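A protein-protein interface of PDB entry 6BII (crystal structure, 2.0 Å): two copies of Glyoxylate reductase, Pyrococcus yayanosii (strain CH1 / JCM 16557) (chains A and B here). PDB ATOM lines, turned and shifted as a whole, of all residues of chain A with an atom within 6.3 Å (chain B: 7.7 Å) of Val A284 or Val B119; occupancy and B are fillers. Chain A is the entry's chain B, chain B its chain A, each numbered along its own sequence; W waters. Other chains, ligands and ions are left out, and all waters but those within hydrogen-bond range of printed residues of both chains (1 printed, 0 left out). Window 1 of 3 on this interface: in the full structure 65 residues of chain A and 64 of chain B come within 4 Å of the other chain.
The backbone carbonyl oxygen of Leu A280 sits at hydrogen-bond distance from the guanidinium group of Arg B127 (2.9 Å). The guanidinium group (NH2) of Arg B117 sits at hydrogen-bond distance from the backbone carbonyl oxygen (O) of Ile A289, at 2.9 Å. OD2 of Asp B123 lies within hydrogen-bond range of N of Leu A285 (2.8 Å). NH2 of Arg B127 is in hydrogen-bond range of O of Val A283, at 2.8 Å.
The backbone carbonyl oxygen (O) of Val A284 is in hydrogen-bond range of the backbone NH (N) of Leu A264 (2.9 Å). OD1 of Asp A265 lies within hydrogen-bond range of N of Ile A289, at 2.8 Å. The backbone carbonyl oxygen (O) of Leu A264 lies within hydrogen-bond range of the backbone NH (N) of Thr A286. The backbone NH of Val A284 is in hydrogen-bond range of the backbone carbonyl oxygen of Ala A262 (2.9 Å). OD1 of Asp B123 lies within salt-bridge range of NE of Arg B127, 2.8 Å away. The backbone NH (N) of Val B119 is in hydrogen-bond range of the backbone carbonyl oxygen (O) of Ala B114.
Among the printed residues, merely in contact across the chains: Val A284 with Asp B123, Val A120 with Asp B123, Ala A110 with Leu B113, Ile A289 with Phe B143, Leu A285 with Gly B122, Leu A107 with Arg B117, Thr A286 with Val B126, Val A119 with Val B284, Leu A285 with Val B126, Val A119 with Ala B110, Val A284 with Val B119 and Ala A110 with Val B119.
Printed residues of chain B within 4 Å of Val A120: Asp B123 (3.6 Å). Val A284 touches just these residues of chain B: Val B119 (3.9 Å) and Asp B123 (3.5 Å). Of the printed residues of chain B, Ile A289 touches Arg B117 (2.9 Å) and Phe B143 (3.7 Å). Of chain A, only Ala A110 (3.9 Å) and Val A284 (3.9 Å) come within 4 Å of Val B119. Of the printed residues of chain A, Arg B127 touches Leu A280 and Val A283. Asp B281 touches none of the printed residues of chain A. The nearest residue of chain A that does not touch Val B119 is Leu A285 (4.2 Å). The nearest printed residue of chain A that does not touch Arg B117 is Ala A110 (5.0 Å).
Of the 21 printed residues of chain A, 10 touch a printed residue of chain B. Printed residues of chain A that touch a printed residue of chain B: Leu A107, Ala A110, Val A119, Val A120, Leu A280, Val A283, Val A284, Leu A285, Thr A286 and Ile A289. Among the printed residues, 16 pairs touch across the chains.
Ala A110 touches Val B119, and with the chains exchanged Val A119 touches Ala B110. Val A119 touches Val B284, and with the chains exchanged Val A284 touches Val B119. Of the 16 pairs that touch across the chains among the printed residues, 4 have their exchanged pair printed and touching as well.
Water W1 lies within hydrogen-bond range of the backbone carbonyl oxygen (O) of Ala A110 and the backbone carbonyl oxygen (O) of Ala B110.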
ATOM      1  N   LEU A 107     -26.593  18.082  -3.138  1.00  0.00           N
ATOM      2  CA  LEU A 107     -26.128  18.372  -1.771  1.00  0.00           C
ATOM      3  C   LEU A 107     -26.636  19.714  -1.275  1.00  0.00           C
ATOM      4  O   LEU A 107     -27.056  19.829  -0.101  1.00  0.00           O
ATOM      5  CB  LEU A 107     -24.601  18.250  -1.622  1.00  0.00           C
ATOM      6  CG  LEU A 107     -24.294  18.446  -0.132  1.00  0.00           C
ATOM      7  CD1 LEU A 107     -24.546  17.155   0.615  1.00  0.00           C
ATOM      8  CD2 LEU A 107     -23.017  19.097   0.234  1.00  0.00           C
ATOM      9  N   ALA A 110     -30.042  19.115  -0.193  1.00  0.00           N
ATOM     10  CA  ALA A 110     -30.045  18.355   1.069  1.00  0.00           C
ATOM     11  C   ALA A 110     -29.859  19.301   2.251  1.00  0.00           C
ATOM     12  O   ALA A 110     -30.562  19.214   3.233  1.00  0.00           O
ATOM     13  CB  ALA A 110     -28.942  17.300   1.065  1.00  0.00           C
ATOM     14  N   LEU A 111     -28.918  20.218   2.127  1.00  0.00           N
ATOM     15  CA  LEU A 111     -28.661  21.210   3.161  1.00  0.00           C
ATOM     16  C   LEU A 111     -29.814  22.179   3.354  1.00  0.00           C
ATOM     17  O   LEU A 111     -30.202  22.471   4.470  1.00  0.00           O
ATOM     18  CB  LEU A 111     -27.378  21.963   2.871  1.00  0.00           C
ATOM     19  CG  LEU A 111     -26.090  21.153   3.030  1.00  0.00           C
ATOM     20  CD1 LEU A 111     -24.908  21.969   2.542  1.00  0.00           C
ATOM     21  CD2 LEU A 111     -25.882  20.761   4.485  1.00  0.00           C
ATOM     22  N   ALA A 114     -32.612  20.227   5.128  1.00  0.00           N
ATOM     23  CA  ALA A 114     -32.219  19.865   6.495  1.00  0.00           C
ATOM     24  C   ALA A 114     -32.286  21.049   7.427  1.00  0.00           C
ATOM     25  O   ALA A 114     -32.844  20.964   8.525  1.00  0.00           O
ATOM     26  CB  ALA A 114     -30.828  19.244   6.514  1.00  0.00           C
ATOM     27  N   ALA A 115     -31.755  22.179   6.977  1.00  0.00           N
ATOM     28  CA  ALA A 115     -31.777  23.393   7.791  1.00  0.00           C
ATOM     29  C   ALA A 115     -33.183  23.918   7.935  1.00  0.00           C
ATOM     30  O   ALA A 115     -33.561  24.384   8.995  1.00  0.00           O
ATOM     31  CB  ALA A 115     -30.860  24.453   7.178  1.00  0.00           C
ATOM     32  N   ALA A 116     -33.975  23.846   6.871  1.00  0.00           N
ATOM     33  CA  ALA A 116     -35.345  24.357   6.920  1.00  0.00           C
ATOM     34  C   ALA A 116     -36.249  23.610   7.867  1.00  0.00           C
ATOM     35  O   ALA A 116     -37.140  24.219   8.465  1.00  0.00           O
ATOM     36  CB  ALA A 116     -35.949  24.321   5.539  1.00  0.00           C
ATOM     37  N   VAL A 119     -33.791  18.719  10.456  1.00  0.00           N
ATOM     38  CA  VAL A 119     -33.493  17.285  10.346  1.00  0.00           C
ATOM     39  C   VAL A 119     -32.360  16.814  11.263  1.00  0.00           C
ATOM     40  O   VAL A 119     -32.484  15.761  11.874  1.00  0.00           O
ATOM     41  CB  VAL A 119     -33.192  16.882   8.897  1.00  0.00           C
ATOM     42  CG1 VAL A 119     -32.725  15.434   8.801  1.00  0.00           C
ATOM     43  CG2 VAL A 119     -34.449  17.074   8.066  1.00  0.00           C
ATOM     44  N   VAL A 120     -31.285  17.586  11.382  1.00  0.00           N
ATOM     45  CA  VAL A 120     -30.177  17.218  12.276  1.00  0.00           C
ATOM     46  C   VAL A 120     -30.586  17.238  13.746  1.00  0.00           C
ATOM     47  O   VAL A 120     -30.336  16.298  14.499  1.00  0.00           O
ATOM     48  CB  VAL A 120     -28.942  18.082  11.986  1.00  0.00           C
ATOM     49  CG1 VAL A 120     -27.873  17.923  13.073  1.00  0.00           C
ATOM     50  CG2 VAL A 120     -28.399  17.711  10.601  1.00  0.00           C
ATOM     51  N   ALA A 262     -28.678  28.135   8.654  1.00  0.00           N
ATOM     52  CA  ALA A 262     -27.731  27.965   7.595  1.00  0.00           C
ATOM     53  C   ALA A 262     -27.308  26.514   7.458  1.00  0.00           C
ATOM     54  O   ALA A 262     -27.253  25.793   8.432  1.00  0.00           O
ATOM     55  CB  ALA A 262     -26.511  28.835   7.804  1.00  0.00           C
ATOM     56  N   GLY A 263     -26.984  26.137   6.219  1.00  0.00           N
ATOM     57  CA  GLY A 263     -26.421  24.847   5.864  1.00  0.00           C
ATOM     58  C   GLY A 263     -25.107  25.144   5.192  1.00  0.00           C
ATOM     59  O   GLY A 263     -25.075  25.815   4.156  1.00  0.00           O
ATOM     60  N   LEU A 264     -24.027  24.617   5.752  1.00  0.00           N
ATOM     61  CA  LEU A 264     -22.684  24.912   5.266  1.00  0.00           C
ATOM     62  C   LEU A 264     -21.870  23.665   4.934  1.00  0.00           C
ATOM     63  O   LEU A 264     -21.684  22.794   5.782  1.00  0.00           O
ATOM     64  CB  LEU A 264     -21.924  25.685   6.376  1.00  0.00           C
ATOM     65  CG  LEU A 264     -22.622  26.934   6.946  1.00  0.00           C
ATOM     66  CD1 LEU A 264     -21.813  27.491   8.116  1.00  0.00           C
ATOM     67  CD2 LEU A 264     -22.826  27.994   5.860  1.00  0.00           C
ATOM     68  N   ASP A 265     -21.393  23.584   3.697  1.00  0.00           N
ATOM     69  CA  ASP A 265     -20.536  22.508   3.256  1.00  0.00           C
ATOM     70  C   ASP A 265     -19.066  22.914   3.225  1.00  0.00           C
ATOM     71  O   ASP A 265     -18.203  22.059   3.101  1.00  0.00           O
ATOM     72  CB  ASP A 265     -20.939  22.043   1.842  1.00  0.00           C
ATOM     73  CG  ASP A 265     -20.228  20.781   1.419  1.00  0.00           C
ATOM     74  OD1 ASP A 265     -20.278  19.766   2.180  1.00  0.00           O
ATOM     75  OD2 ASP A 265     -19.599  20.784   0.327  1.00  0.00           O
ATOM     76  N   PHE A 267     -15.901  26.018   4.404  1.00  0.00           N
ATOM     77  CA  PHE A 267     -15.444  26.847   5.537  1.00  0.00           C
ATOM     78  C   PHE A 267     -14.168  27.587   5.160  1.00  0.00           C
ATOM     79  O   PHE A 267     -13.456  27.177   4.231  1.00  0.00           O
ATOM     80  CB  PHE A 267     -15.224  25.969   6.796  1.00  0.00           C
ATOM     81  CG  PHE A 267     -16.428  25.165   7.162  1.00  0.00           C
ATOM     82  CD1 PHE A 267     -16.684  23.946   6.532  1.00  0.00           C
ATOM     83  CD2 PHE A 267     -17.370  25.676   8.031  1.00  0.00           C
ATOM     84  CE1 PHE A 267     -17.831  23.228   6.811  1.00  0.00           C
ATOM     85  CE2 PHE A 267     -18.533  24.969   8.321  1.00  0.00           C
ATOM     86  CZ  PHE A 267     -18.757  23.725   7.714  1.00  0.00           C
ATOM     87  N   LEU A 280     -24.566  25.895  17.859  1.00  0.00           N
ATOM     88  CA  LEU A 280     -25.869  26.417  17.427  1.00  0.00           C
ATOM     89  C   LEU A 280     -26.756  25.339  16.813  1.00  0.00           C
ATOM     90  O   LEU A 280     -26.329  24.572  15.956  1.00  0.00           O
ATOM     91  CB  LEU A 280     -25.664  27.563  16.423  1.00  0.00           C
ATOM     92  CG  LEU A 280     -24.847  28.742  17.003  1.00  0.00           C
ATOM     93  CD1 LEU A 280     -24.675  29.829  15.999  1.00  0.00           C
ATOM     94  CD2 LEU A 280     -25.431  29.332  18.287  1.00  0.00           C
ATOM     95  N   ASP A 281     -28.000  25.295  17.264  1.00  0.00           N
ATOM     96  CA  ASP A 281     -28.998  24.357  16.699  1.00  0.00           C
ATOM     97  C   ASP A 281     -29.465  24.707  15.312  1.00  0.00           C
ATOM     98  O   ASP A 281     -30.046  23.856  14.630  1.00  0.00           O
ATOM     99  CB  ASP A 281     -30.261  24.362  17.564  1.00  0.00           C
ATOM    100  CG  ASP A 281     -30.081  23.594  18.820  1.00  0.00           C
ATOM    101  OD1 ASP A 281     -29.279  22.607  18.808  1.00  0.00           O
ATOM    102  OD2 ASP A 281     -30.729  24.009  19.809  1.00  0.00           O
ATOM    103  N   ASN A 282     -29.273  25.968  14.918  1.00  0.00           N
ATOM    104  CA  ASN A 282     -29.776  26.434  13.620  1.00  0.00           C
ATOM    105  C   ASN A 282     -28.684  26.463  12.549  1.00  0.00           C
ATOM    106  O   ASN A 282     -28.814  27.180  11.552  1.00  0.00           O
ATOM    107  CB  ASN A 282     -30.513  27.773  13.752  1.00  0.00           C
ATOM    108  CG  ASN A 282     -29.650  28.893  14.315  1.00  0.00           C
ATOM    109  OD1 ASN A 282     -28.625  28.622  14.947  1.00  0.00           O
ATOM    110  ND2 ASN A 282     -30.087  30.163  14.109  1.00  0.00           N
ATOM    111  N   VAL A 283     -27.630  25.672  12.734  1.00  0.00           N
ATOM    112  CA  VAL A 283     -26.670  25.398  11.637  1.00  0.00           C
ATOM    113  C   VAL A 283     -26.659  23.902  11.345  1.00  0.00           C
ATOM    114  O   VAL A 283     -26.831  23.101  12.260  1.00  0.00           O
ATOM    115  CB  VAL A 283     -25.247  25.940  11.935  1.00  0.00           C
ATOM    116  CG1 VAL A 283     -24.505  25.129  12.984  1.00  0.00           C
ATOM    117  CG2 VAL A 283     -24.425  26.019  10.661  1.00  0.00           C
ATOM    118  N   VAL A 284     -26.485  23.560  10.070  1.00  0.00           N
ATOM    119  CA  VAL A 284     -26.278  22.187   9.603  1.00  0.00           C
ATOM    120  C   VAL A 284     -24.937  22.196   8.887  1.00  0.00           C
ATOM    121  O   VAL A 284     -24.673  23.091   8.079  1.00  0.00           O
ATOM    122  CB  VAL A 284     -27.379  21.745   8.622  1.00  0.00           C
ATOM    123  CG1 VAL A 284     -27.032  20.383   8.015  1.00  0.00           C
ATOM    124  CG2 VAL A 284     -28.728  21.724   9.312  1.00  0.00           C
ATOM    125  N   LEU A 285     -24.093  21.208   9.190  1.00  0.00           N
ATOM    126  CA  LEU A 285     -22.688  21.187   8.774  1.00  0.00           C
ATOM    127  C   LEU A 285     -22.380  19.920   7.996  1.00  0.00           C
ATOM    128  O   LEU A 285     -22.819  18.854   8.385  1.00  0.00           O
ATOM    129  CB  LEU A 285     -21.797  21.207  10.021  1.00  0.00           C
ATOM    130  CG  LEU A 285     -22.054  22.363  10.990  1.00  0.00           C
ATOM    131  CD1 LEU A 285     -21.495  22.035  12.381  1.00  0.00           C
ATOM    132  CD2 LEU A 285     -21.453  23.646  10.452  1.00  0.00           C
ATOM    133  N   THR A 286     -21.636  20.039   6.904  1.00  0.00           N
ATOM    134  CA  THR A 286     -21.087  18.854   6.222  1.00  0.00           C
ATOM    135  C   THR A 286     -19.637  19.133   5.882  1.00  0.00           C
ATOM    136  O   THR A 286     -19.264  20.304   5.648  1.00  0.00           O
ATOM    137  CB  THR A 286     -21.899  18.465   4.953  1.00  0.00           C
ATOM    138  OG1 THR A 286     -22.079  19.608   4.107  1.00  0.00           O
ATOM    139  CG2 THR A 286     -23.245  17.951   5.344  1.00  0.00           C
ATOM    140  N   ILE A 289     -18.429  17.930   1.181  1.00  0.00           N
ATOM    141  CA  ILE A 289     -18.816  16.718   0.474  1.00  0.00           C
ATOM    142  C   ILE A 289     -19.741  16.992  -0.716  1.00  0.00           C
ATOM    143  O   ILE A 289     -20.371  16.072  -1.217  1.00  0.00           O
ATOM    144  CB  ILE A 289     -19.459  15.698   1.434  1.00  0.00           C
ATOM    145  CG1 ILE A 289     -20.709  16.253   2.099  1.00  0.00           C
ATOM    146  CG2 ILE A 289     -18.438  15.285   2.473  1.00  0.00           C
ATOM    147  CD1 ILE A 289     -21.568  15.250   2.845  1.00  0.00           C
ATOM    148  N   ALA B 110     -36.614  15.973   2.346  1.00  0.00           N
ATOM    149  CA  ALA B 110     -35.525  16.244   3.290  1.00  0.00           C
ATOM    150  C   ALA B 110     -34.866  14.932   3.752  1.00  0.00           C
ATOM    151  O   ALA B 110     -33.655  14.800   3.761  1.00  0.00           O
ATOM    152  CB  ALA B 110     -36.032  17.024   4.502  1.00  0.00           C
ATOM    153  N   LEU B 113     -32.885  13.025   0.765  1.00  0.00           N
ATOM    154  CA  LEU B 113     -31.580  13.616   0.486  1.00  0.00           C
ATOM    155  C   LEU B 113     -30.603  13.456   1.650  1.00  0.00           C
ATOM    156  O   LEU B 113     -29.424  13.176   1.439  1.00  0.00           O
ATOM    157  CB  LEU B 113     -31.734  15.094   0.110  1.00  0.00           C
ATOM    158  CG  LEU B 113     -32.333  15.263  -1.288  1.00  0.00           C
ATOM    159  CD1 LEU B 113     -32.905  16.673  -1.418  1.00  0.00           C
ATOM    160  CD2 LEU B 113     -31.287  15.020  -2.375  1.00  0.00           C
ATOM    161  N   ALA B 114     -31.091  13.586   2.873  1.00  0.00           N
ATOM    162  CA  ALA B 114     -30.199  13.423   4.042  1.00  0.00           C
ATOM    163  C   ALA B 114     -29.657  12.000   4.109  1.00  0.00           C
ATOM    164  O   ALA B 114     -28.462  11.795   4.344  1.00  0.00           O
ATOM    165  CB  ALA B 114     -30.922  13.778   5.332  1.00  0.00           C
ATOM    166  N   ALA B 115     -30.527  11.019   3.895  1.00  0.00           N
ATOM    167  CA  ALA B 115     -30.103   9.620   3.932  1.00  0.00           C
ATOM    168  C   ALA B 115     -29.211   9.293   2.753  1.00  0.00           C
ATOM    169  O   ALA B 115     -28.249   8.557   2.894  1.00  0.00           O
ATOM    170  CB  ALA B 115     -31.316   8.697   3.927  1.00  0.00           C
ATOM    171  N   ALA B 116     -29.512   9.843   1.592  1.00  0.00           N
ATOM    172  CA  ALA B 116     -28.709   9.581   0.400  1.00  0.00           C
ATOM    173  C   ALA B 116     -27.280  10.087   0.501  1.00  0.00           C
ATOM    174  O   ALA B 116     -26.367   9.465  -0.077  1.00  0.00           O
ATOM    175  CB  ALA B 116     -29.360  10.203  -0.816  1.00  0.00           C
ATOM    176  N   ARG B 117     -27.095  11.243   1.163  1.00  0.00           N
ATOM    177  CA  ARG B 117     -25.821  11.959   1.154  1.00  0.00           C
ATOM    178  C   ARG B 117     -25.121  12.096   2.514  1.00  0.00           C
ATOM    179  O   ARG B 117     -24.139  12.829   2.653  1.00  0.00           O
ATOM    180  CB  ARG B 117     -26.019  13.320   0.489  1.00  0.00           C
ATOM    181  CG  ARG B 117     -26.383  13.219  -1.003  1.00  0.00           C
ATOM    182  CD  ARG B 117     -25.355  12.497  -1.877  1.00  0.00           C
ATOM    183  NE  ARG B 117     -24.141  13.269  -1.856  1.00  0.00           N
ATOM    184  CZ  ARG B 117     -23.884  14.329  -2.606  1.00  0.00           C
ATOM    185  NH1 ARG B 117     -24.728  14.710  -3.552  1.00  0.00           N
ATOM    186  NH2 ARG B 117     -22.766  14.988  -2.406  1.00  0.00           N
ATOM    187  N   HIS B 118     -25.589  11.327   3.487  1.00  0.00           N
ATOM    188  CA  HIS B 118     -24.956  11.231   4.812  1.00  0.00           C
ATOM    189  C   HIS B 118     -24.927  12.557   5.578  1.00  0.00           C
ATOM    190  O   HIS B 118     -23.955  12.841   6.269  1.00  0.00           O
ATOM    191  CB  HIS B 118     -23.522  10.688   4.712  1.00  0.00           C
ATOM    192  CG  HIS B 118     -23.366   9.483   3.840  1.00  0.00           C
ATOM    193  ND1 HIS B 118     -23.913   8.253   4.154  1.00  0.00           N
ATOM    194  CD2 HIS B 118     -22.682   9.314   2.677  1.00  0.00           C
ATOM    195  CE1 HIS B 118     -23.590   7.391   3.203  1.00  0.00           C
ATOM    196  NE2 HIS B 118     -22.831   8.005   2.305  1.00  0.00           N
ATOM    197  N   VAL B 119     -25.984  13.354   5.467  1.00  0.00           N
ATOM    198  CA  VAL B 119     -26.009  14.680   6.114  1.00  0.00           C
ATOM    199  C   VAL B 119     -25.934  14.641   7.638  1.00  0.00           C
ATOM    200  O   VAL B 119     -25.194  15.413   8.228  1.00  0.00           O
ATOM    201  CB  VAL B 119     -27.228  15.508   5.664  1.00  0.00           C
ATOM    202  CG1 VAL B 119     -27.353  16.818   6.460  1.00  0.00           C
ATOM    203  CG2 VAL B 119     -27.096  15.808   4.187  1.00  0.00           C
ATOM    204  N   VAL B 120     -26.659  13.725   8.268  1.00  0.00           N
ATOM    205  CA  VAL B 120     -26.650  13.607   9.713  1.00  0.00           C
ATOM    206  C   VAL B 120     -25.291  13.134  10.260  1.00  0.00           C
ATOM    207  O   VAL B 120     -24.725  13.711  11.214  1.00  0.00           O
ATOM    208  CB  VAL B 120     -27.823  12.752  10.201  1.00  0.00           C
ATOM    209  CG1 VAL B 120     -27.706  12.458  11.691  1.00  0.00           C
ATOM    210  CG2 VAL B 120     -29.122  13.486   9.938  1.00  0.00           C
ATOM    211  N   LYS B 121     -24.755  12.099   9.649  1.00  0.00           N
ATOM    212  CA  LYS B 121     -23.451  11.564  10.029  1.00  0.00           C
ATOM    213  C   LYS B 121     -22.361  12.619   9.783  1.00  0.00           C
ATOM    214  O   LYS B 121     -21.458  12.803  10.598  1.00  0.00           O
ATOM    215  CB  LYS B 121     -23.130  10.302   9.224  1.00  0.00           C
ATOM    216  CG  LYS B 121     -22.053   9.396   9.821  1.00  0.00           C
ATOM    217  CD  LYS B 121     -21.348   8.465   8.818  1.00  0.00           C
ATOM    218  CE  LYS B 121     -22.142   8.077   7.559  1.00  0.00           C
ATOM    219  NZ  LYS B 121     -21.329   7.333   6.543  1.00  0.00           N
ATOM    220  N   GLY B 122     -22.456  13.306   8.655  1.00  0.00           N
ATOM    221  CA  GLY B 122     -21.503  14.355   8.329  1.00  0.00           C
ATOM    222  C   GLY B 122     -21.509  15.490   9.324  1.00  0.00           C
ATOM    223  O   GLY B 122     -20.459  15.987   9.715  1.00  0.00           O
ATOM    224  N   ASP B 123     -22.708  15.918   9.711  1.00  0.00           N
ATOM    225  CA  ASP B 123     -22.836  16.978  10.682  1.00  0.00           C
ATOM    226  C   ASP B 123     -22.160  16.593  11.996  1.00  0.00           C
ATOM    227  O   ASP B 123     -21.401  17.390  12.544  1.00  0.00           O
ATOM    228  CB  ASP B 123     -24.287  17.388  10.868  1.00  0.00           C
ATOM    229  CG  ASP B 123     -24.461  18.510  11.889  1.00  0.00           C
ATOM    230  OD1 ASP B 123     -24.291  18.254  13.106  1.00  0.00           O
ATOM    231  OD2 ASP B 123     -24.792  19.663  11.474  1.00  0.00           O
ATOM    232  N   LYS B 124     -22.408  15.387  12.481  1.00  0.00           N
ATOM    233  CA  LYS B 124     -21.801  14.985  13.752  1.00  0.00           C
ATOM    234  C   LYS B 124     -20.259  14.909  13.639  1.00  0.00           C
ATOM    235  O   LYS B 124     -19.538  15.321  14.565  1.00  0.00           O
ATOM    236  CB  LYS B 124     -22.417  13.695  14.260  1.00  0.00           C
ATOM    237  CG  LYS B 124     -21.881  13.155  15.584  1.00  0.00           C
ATOM    238  CD  LYS B 124     -22.065  11.646  15.665  1.00  0.00           C
ATOM    239  CE  LYS B 124     -21.607  11.062  16.997  1.00  0.00           C
ATOM    240  NZ  LYS B 124     -22.574  11.256  18.110  1.00  0.00           N
ATOM    241  N   PHE B 125     -19.789  14.413  12.490  1.00  0.00           N
ATOM    242  CA  PHE B 125     -18.348  14.359  12.189  1.00  0.00           C
ATOM    243  C   PHE B 125     -17.687  15.752  12.298  1.00  0.00           C
ATOM    244  O   PHE B 125     -16.595  15.898  12.875  1.00  0.00           O
ATOM    245  CB  PHE B 125     -18.174  13.764  10.781  1.00  0.00           C
ATOM    246  CG  PHE B 125     -16.749  13.527  10.365  1.00  0.00           C
ATOM    247  CD1 PHE B 125     -15.996  12.504  10.932  1.00  0.00           C
ATOM    248  CD2 PHE B 125     -16.169  14.301   9.371  1.00  0.00           C
ATOM    249  CE1 PHE B 125     -14.708  12.254  10.506  1.00  0.00           C
ATOM    250  CE2 PHE B 125     -14.875  14.060   8.959  1.00  0.00           C
ATOM    251  CZ  PHE B 125     -14.140  13.036   9.524  1.00  0.00           C
ATOM    252  N   VAL B 126     -18.366  16.773  11.780  1.00  0.00           N
ATOM    253  CA  VAL B 126     -17.843  18.156  11.863  1.00  0.00           C
ATOM    254  C   VAL B 126     -18.005  18.726  13.267  1.00  0.00           C
ATOM    255  O   VAL B 126     -17.030  19.225  13.886  1.00  0.00           O
ATOM    256  CB  VAL B 126     -18.540  19.069  10.851  1.00  0.00           C
ATOM    257  CG1 VAL B 126     -18.102  20.528  11.033  1.00  0.00           C
ATOM    258  CG2 VAL B 126     -18.254  18.598   9.422  1.00  0.00           C
ATOM    259  N   ARG B 127     -19.234  18.656  13.761  1.00  0.00           N
ATOM    260  CA  ARG B 127     -19.637  19.318  15.011  1.00  0.00           C
ATOM    261  C   ARG B 127     -18.855  18.839  16.219  1.00  0.00           C
ATOM    262  O   ARG B 127     -18.514  19.647  17.098  1.00  0.00           O
ATOM    263  CB  ARG B 127     -21.138  19.139  15.238  1.00  0.00           C
ATOM    264  CG  ARG B 127     -21.752  20.062  16.279  1.00  0.00           C
ATOM    265  CD  ARG B 127     -23.243  19.776  16.406  1.00  0.00           C
ATOM    266  NE  ARG B 127     -23.965  20.082  15.174  1.00  0.00           N
ATOM    267  CZ  ARG B 127     -24.561  21.243  14.900  1.00  0.00           C
ATOM    268  NH1 ARG B 127     -24.565  22.252  15.752  1.00  0.00           N
ATOM    269  NH2 ARG B 127     -25.202  21.382  13.763  1.00  0.00           N
ATOM    270  N   PHE B 143     -17.091  10.208   2.513  1.00  0.00           N
ATOM    271  CA  PHE B 143     -18.556  10.363   2.626  1.00  0.00           C
ATOM    272  C   PHE B 143     -19.279  10.228   1.262  1.00  0.00           C
ATOM    273  O   PHE B 143     -20.261  10.936   0.970  1.00  0.00           O
ATOM    274  CB  PHE B 143     -18.915  11.711   3.336  1.00  0.00           C
ATOM    275  CG  PHE B 143     -18.840  11.663   4.831  1.00  0.00           C
ATOM    276  CD1 PHE B 143     -19.836  11.076   5.562  1.00  0.00           C
ATOM    277  CD2 PHE B 143     -17.750  12.154   5.514  1.00  0.00           C
ATOM    278  CE1 PHE B 143     -19.763  11.019   6.939  1.00  0.00           C
ATOM    279  CE2 PHE B 143     -17.662  12.091   6.896  1.00  0.00           C
ATOM    280  CZ  PHE B 143     -18.670  11.529   7.613  1.00  0.00           C
ATOM    281  N   ASP B 281     -25.396   4.174  11.285  1.00  0.00           N
ATOM    282  CA  ASP B 281     -25.037   5.374  10.515  1.00  0.00           C
ATOM    283  C   ASP B 281     -25.892   5.618   9.278  1.00  0.00           C
ATOM    284  O   ASP B 281     -25.925   6.717   8.762  1.00  0.00           O
ATOM    285  CB  ASP B 281     -23.606   5.194  10.013  1.00  0.00           C
ATOM    286  CG  ASP B 281     -22.598   5.495  11.059  1.00  0.00           C
ATOM    287  OD1 ASP B 281     -22.918   6.111  12.105  1.00  0.00           O
ATOM    288  OD2 ASP B 281     -21.449   5.166  10.793  1.00  0.00           O
ATOM    289  N   VAL B 284     -31.616   7.865   9.083  1.00  0.00           N
ATOM    290  CA  VAL B 284     -31.879   9.256   9.458  1.00  0.00           C
ATOM    291  C   VAL B 284     -33.259   9.265  10.094  1.00  0.00           C
ATOM    292  O   VAL B 284     -34.179   8.639   9.545  1.00  0.00           O
ATOM    293  CB  VAL B 284     -31.879  10.183   8.236  1.00  0.00           C
ATOM    294  CG1 VAL B 284     -32.347  11.580   8.623  1.00  0.00           C
ATOM    295  CG2 VAL B 284     -30.486  10.250   7.652  1.00  0.00           C
HETATM  296  O   HOH W   1     -31.801  16.881   4.197  1.00  0.00           O
